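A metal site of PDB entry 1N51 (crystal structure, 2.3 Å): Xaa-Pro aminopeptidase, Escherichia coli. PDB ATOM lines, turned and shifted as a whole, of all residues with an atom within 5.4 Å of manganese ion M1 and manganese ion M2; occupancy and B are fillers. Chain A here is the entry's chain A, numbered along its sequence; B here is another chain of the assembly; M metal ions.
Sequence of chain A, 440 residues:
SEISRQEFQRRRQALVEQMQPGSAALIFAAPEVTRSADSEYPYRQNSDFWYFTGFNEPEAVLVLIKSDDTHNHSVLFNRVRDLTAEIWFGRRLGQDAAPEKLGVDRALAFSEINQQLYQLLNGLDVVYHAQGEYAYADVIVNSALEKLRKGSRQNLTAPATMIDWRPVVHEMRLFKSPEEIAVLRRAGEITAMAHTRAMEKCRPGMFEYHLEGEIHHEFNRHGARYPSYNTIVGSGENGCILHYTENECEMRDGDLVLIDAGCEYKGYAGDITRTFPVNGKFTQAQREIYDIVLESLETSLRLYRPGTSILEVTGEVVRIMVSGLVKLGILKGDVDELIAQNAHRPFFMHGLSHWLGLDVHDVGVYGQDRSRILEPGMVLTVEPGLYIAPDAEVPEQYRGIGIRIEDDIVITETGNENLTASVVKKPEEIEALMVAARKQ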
ATOM      1  N   TYR A 229      24.266  -8.200 -28.444  1.00  0.00           N
ATOM      2  CA  TYR A 229      25.568  -7.829 -29.019  1.00  0.00           C
ATOM      3  C   TYR A 229      26.650  -8.473 -28.161  1.00  0.00           C
ATOM      4  O   TYR A 229      26.382  -8.874 -27.030  1.00  0.00           O
ATOM      5  CB  TYR A 229      25.768  -6.311 -29.064  1.00  0.00           C
ATOM      6  CG  TYR A 229      25.584  -5.613 -27.739  1.00  0.00           C
ATOM      7  CD1 TYR A 229      24.315  -5.203 -27.327  1.00  0.00           C
ATOM      8  CD2 TYR A 229      26.659  -5.400 -26.865  1.00  0.00           C
ATOM      9  CE1 TYR A 229      24.117  -4.596 -26.081  1.00  0.00           C
ATOM     10  CE2 TYR A 229      26.478  -4.805 -25.626  1.00  0.00           C
ATOM     11  CZ  TYR A 229      25.198  -4.396 -25.237  1.00  0.00           C
ATOM     12  OH  TYR A 229      24.988  -3.801 -24.008  1.00  0.00           O
ATOM     13  N   ASP A 260      29.591  -3.527 -20.715  1.00  0.00           N
ATOM     14  CA  ASP A 260      28.549  -3.118 -21.632  1.00  0.00           C
ATOM     15  C   ASP A 260      27.957  -4.442 -22.109  1.00  0.00           C
ATOM     16  O   ASP A 260      28.605  -5.199 -22.838  1.00  0.00           O
ATOM     17  CB  ASP A 260      29.130  -2.335 -22.804  1.00  0.00           C
ATOM     18  CG  ASP A 260      28.067  -1.542 -23.568  1.00  0.00           C
ATOM     19  OD1 ASP A 260      26.861  -1.855 -23.456  1.00  0.00           O
ATOM     20  OD2 ASP A 260      28.446  -0.612 -24.313  1.00  0.00           O
ATOM     21  N   ASP A 271      20.416  -2.721 -23.505  1.00  0.00           N
ATOM     22  CA  ASP A 271      21.756  -2.190 -23.739  1.00  0.00           C
ATOM     23  C   ASP A 271      22.184  -1.343 -22.563  1.00  0.00           C
ATOM     24  O   ASP A 271      21.885  -0.155 -22.496  1.00  0.00           O
ATOM     25  CB  ASP A 271      21.776  -1.343 -25.021  1.00  0.00           C
ATOM     26  CG  ASP A 271      23.163  -0.807 -25.343  1.00  0.00           C
ATOM     27  OD1 ASP A 271      24.125  -1.148 -24.609  1.00  0.00           O
ATOM     28  OD2 ASP A 271      23.304  -0.049 -26.326  1.00  0.00           O
ATOM     29  N   ILE A 272      22.885  -1.959 -21.618  1.00  0.00           N
ATOM     30  CA  ILE A 272      23.339  -1.257 -20.433  1.00  0.00           C
ATOM     31  C   ILE A 272      24.864  -1.291 -20.259  1.00  0.00           C
ATOM     32  O   ILE A 272      25.533  -2.270 -20.595  1.00  0.00           O
ATOM     33  CB  ILE A 272      22.714  -1.877 -19.155  1.00  0.00           C
ATOM     34  CG1 ILE A 272      21.207  -1.621 -19.130  1.00  0.00           C
ATOM     35  CG2 ILE A 272      23.390  -1.299 -17.904  1.00  0.00           C
ATOM     36  CD1 ILE A 272      20.496  -2.328 -17.979  1.00  0.00           C
ATOM     37  N   THR A 273      25.392  -0.188 -19.741  1.00  0.00           N
ATOM     38  CA  THR A 273      26.804  -0.088 -19.436  1.00  0.00           C
ATOM     39  C   THR A 273      26.908   0.409 -18.008  1.00  0.00           C
ATOM     40  O   THR A 273      26.242   1.390 -17.629  1.00  0.00           O
ATOM     41  CB  THR A 273      27.583   0.894 -20.333  1.00  0.00           C
ATOM     42  OG1 THR A 273      27.481   0.517 -21.708  1.00  0.00           O
ATOM     43  CG2 THR A 273      29.064   0.873 -19.925  1.00  0.00           C
ATOM     44  N   HIS A 354      21.745   6.402 -29.350  1.00  0.00           N
ATOM     45  CA  HIS A 354      21.416   5.741 -30.605  1.00  0.00           C
ATOM     46  C   HIS A 354      20.055   5.078 -30.420  1.00  0.00           C
ATOM     47  O   HIS A 354      19.665   4.742 -29.297  1.00  0.00           O
ATOM     48  CB  HIS A 354      22.484   4.698 -30.995  1.00  0.00           C
ATOM     49  CG  HIS A 354      22.658   3.579 -30.016  1.00  0.00           C
ATOM     50  ND1 HIS A 354      21.751   2.565 -29.822  1.00  0.00           N
ATOM     51  CD2 HIS A 354      23.695   3.310 -29.172  1.00  0.00           C
ATOM     52  CE1 HIS A 354      22.241   1.733 -28.890  1.00  0.00           C
ATOM     53  NE2 HIS A 354      23.418   2.141 -28.460  1.00  0.00           N
ATOM     54  N   VAL A 360      20.364  -3.470 -31.632  1.00  0.00           N
ATOM     55  CA  VAL A 360      20.902  -2.607 -30.595  1.00  0.00           C
ATOM     56  C   VAL A 360      21.144  -1.202 -31.147  1.00  0.00           C
ATOM     57  O   VAL A 360      20.809  -0.214 -30.509  1.00  0.00           O
ATOM     58  CB  VAL A 360      22.164  -3.226 -29.947  1.00  0.00           C
ATOM     59  CG1 VAL A 360      23.258  -3.431 -30.982  1.00  0.00           C
ATOM     60  CG2 VAL A 360      22.631  -2.354 -28.793  1.00  0.00           C
ATOM     61  N   HIS A 361      21.742  -1.110 -32.338  1.00  0.00           N
ATOM     62  CA  HIS A 361      21.917   0.199 -32.981  1.00  0.00           C
ATOM     63  C   HIS A 361      20.765   0.196 -33.966  1.00  0.00           C
ATOM     64  O   HIS A 361      20.934  -0.121 -35.145  1.00  0.00           O
ATOM     65  CB  HIS A 361      23.233   0.256 -33.765  1.00  0.00           C
ATOM     66  CG  HIS A 361      24.454   0.344 -32.890  1.00  0.00           C
ATOM     67  ND1 HIS A 361      25.725   0.149 -33.378  1.00  0.00           N
ATOM     68  CD2 HIS A 361      24.591   0.623 -31.577  1.00  0.00           C
ATOM     69  CE1 HIS A 361      26.595   0.300 -32.394  1.00  0.00           C
ATOM     70  NE2 HIS A 361      25.929   0.592 -31.297  1.00  0.00           N
ATOM     71  N   THR A 381      19.267   5.144 -26.305  1.00  0.00           N
ATOM     72  CA  THR A 381      20.188   4.957 -25.194  1.00  0.00           C
ATOM     73  C   THR A 381      20.747   6.311 -24.787  1.00  0.00           C
ATOM     74  O   THR A 381      20.671   7.282 -25.528  1.00  0.00           O
ATOM     75  CB  THR A 381      21.392   4.054 -25.595  1.00  0.00           C
ATOM     76  OG1 THR A 381      22.165   4.706 -26.612  1.00  0.00           O
ATOM     77  CG2 THR A 381      20.884   2.722 -26.123  1.00  0.00           C
ATOM     78  N   GLU A 383      24.314   7.276 -23.187  1.00  0.00           N
ATOM     79  CA  GLU A 383      25.578   6.703 -22.755  1.00  0.00           C
ATOM     80  C   GLU A 383      26.831   7.571 -22.783  1.00  0.00           C
ATOM     81  O   GLU A 383      27.740   7.323 -23.574  1.00  0.00           O
ATOM     82  CB  GLU A 383      25.838   5.425 -23.548  1.00  0.00           C
ATOM     83  CG  GLU A 383      25.776   5.617 -25.060  1.00  0.00           C
ATOM     84  CD  GLU A 383      25.896   4.304 -25.812  1.00  0.00           C
ATOM     85  OE1 GLU A 383      26.894   3.600 -25.579  1.00  0.00           O
ATOM     86  OE2 GLU A 383      25.004   3.976 -26.630  1.00  0.00           O
ATOM     87  N   ARG A 404      31.952   4.481 -18.683  1.00  0.00           N
ATOM     88  CA  ARG A 404      30.747   4.734 -19.465  1.00  0.00           C
ATOM     89  C   ARG A 404      29.584   4.253 -18.621  1.00  0.00           C
ATOM     90  O   ARG A 404      29.665   3.214 -17.954  1.00  0.00           O
ATOM     91  CB  ARG A 404      30.765   3.995 -20.810  1.00  0.00           C
ATOM     92  CG  ARG A 404      29.434   4.111 -21.572  1.00  0.00           C
ATOM     93  CD  ARG A 404      29.521   3.733 -23.067  1.00  0.00           C
ATOM     94  NE  ARG A 404      29.710   2.302 -23.300  1.00  0.00           N
ATOM     95  CZ  ARG A 404      30.867   1.747 -23.648  1.00  0.00           C
ATOM     96  NH1 ARG A 404      31.950   2.497 -23.815  1.00  0.00           N
ATOM     97  NH2 ARG A 404      30.943   0.433 -23.852  1.00  0.00           N
ATOM     98  N   GLU A 406      25.474   3.738 -19.169  1.00  0.00           N
ATOM     99  CA  GLU A 406      24.420   3.774 -20.163  1.00  0.00           C
ATOM    100  C   GLU A 406      23.074   3.194 -19.743  1.00  0.00           C
ATOM    101  O   GLU A 406      23.013   2.091 -19.204  1.00  0.00           O
ATOM    102  CB  GLU A 406      24.929   3.063 -21.419  1.00  0.00           C
ATOM    103  CG  GLU A 406      23.858   2.530 -22.367  1.00  0.00           C
ATOM    104  CD  GLU A 406      24.442   1.840 -23.586  1.00  0.00           C
ATOM    105  OE1 GLU A 406      25.407   1.057 -23.410  1.00  0.00           O
ATOM    106  OE2 GLU A 406      23.944   2.069 -24.713  1.00  0.00           O
ATOM    107  CB  01B B   1      27.072  -0.986 -27.765  1.00  0.00           C
ATOM    108  CA  01B B   1      27.367   0.362 -27.088  1.00  0.00           C
ATOM    109  N   01B B   1      26.570  -1.974 -26.759  1.00  0.00           N
ATOM    110  O2  01B B   1      26.246   0.786 -26.282  1.00  0.00           O
ATOM    111  C   01B B   1      27.670   1.434 -28.134  1.00  0.00           C
ATOM    112  C6  01B B   1      28.348  -1.517 -28.444  1.00  0.00           C
ATOM    113  C7  01B B   1      28.093  -2.513 -29.555  1.00  0.00           C
ATOM    114  C8  01B B   1      28.916  -3.637 -29.705  1.00  0.00           C
ATOM    115  C9  01B B   1      28.745  -4.513 -30.777  1.00  0.00           C
ATOM    116  C10 01B B   1      27.746  -4.282 -31.724  1.00  0.00           C
ATOM    117  C11 01B B   1      26.917  -3.176 -31.584  1.00  0.00           C
ATOM    118  C12 01B B   1      27.099  -2.298 -30.504  1.00  0.00           C
ATOM    119  O   01B B   1      26.924   1.614 -29.095  1.00  0.00           O
ATOM    120  N   PRO B   2      28.784   2.161 -27.943  1.00  0.00           N
ATOM    121  CA  PRO B   2      29.222   3.232 -28.834  1.00  0.00           C
ATOM    122  C   PRO B   2      28.958   2.975 -30.306  1.00  0.00           C
ATOM    123  O   PRO B   2      29.570   2.106 -30.924  1.00  0.00           O
ATOM    124  CB  PRO B   2      30.698   3.352 -28.500  1.00  0.00           C
ATOM    125  CG  PRO B   2      30.685   3.150 -27.017  1.00  0.00           C
ATOM    126  CD  PRO B   2      29.787   1.940 -26.872  1.00  0.00           C
HETATM  127 MN    MN M   1      26.045  -0.382 -24.825  1.00  0.00          MN
HETATM  128 MN    MN M   2      24.299   1.753 -26.629  1.00  0.00          MN
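OG1 of Thr 381 sits close to OE2 of Glu 383, 2.9 Å away.
NE of Arg 404 lies within salt-bridge range of OE1 of Glu 383 (3.8 Å).
O of 01B 1 of chain B lies within hydrogen-bond range of a ring nitrogen (NE2) of His 361.
The backbone NH (N) of Glu 406 lies within hydrogen-bond range of the backbone carbonyl oxygen (O) of Thr 273.
ND1 of His 354 lies close to O of Val 360, 3.0 Å away.
The backbone NH (N) of Thr 381 sits at hydrogen-bond distance from the backbone carbonyl oxygen (O) of His 354, 3.0 Å away.
The side-chain hydroxyl (OG1) of Thr 273 lies within hydrogen-bond range of the guanidinium group (NE) of Arg 404 (3.3 Å).
The side-chain hydroxyl (OG1) of Thr 273 lies close to the side-chain carboxylate (OD2) of Asp 260, at 3.0 Å.
Tyr 229 touches manganese ion M1 (OH to MN, 3.7 Å).
Thr 273 touches manganese ion M1.
The nearest printed residue that does not touch manganese ion M1 is Glu 383 (4.1 Å).
Residues that only touch manganese ion M2: Thr 381 (3.6 Å).
The nearest printed residue that does not touch manganese ion M2 is Pro 2 of chain B (4.7 Å).
Manganese ion M2 is bound by OE2 of Glu 406, 2.0 Å away.
Manganese ion M2 is bound by NE2 of His 354 (2.1 Å).
OD2 of Asp 271 is bound to manganese ion M2, at 2.1 Å.
Manganese ion M2 is bound by O2 of 01B 1 of chain B (2.2 Å).
The side-chain carboxylate (OE2) of Glu 383 binds manganese ion M2.
Manganese ion M2 has five donor atoms within binding distance.
Manganese ion M1 is bound by O2 of 01B 1 of chain B.
OD1 of Asp 271 binds manganese ion M1 (2.1 Å).
Manganese ion M1 is bound by OE1 of Glu 406 (2.1 Å).
The side-chain carboxylate (OD1) of Asp 260 binds manganese ion M1 (2.2 Å).
OD2 of Asp 260 is bound to manganese ion M1, 2.5 Å away.
N of 01B 1 of chain B binds manganese ion M1, at 2.6 Å.
Manganese ion M1 has six donor atoms within binding distance.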
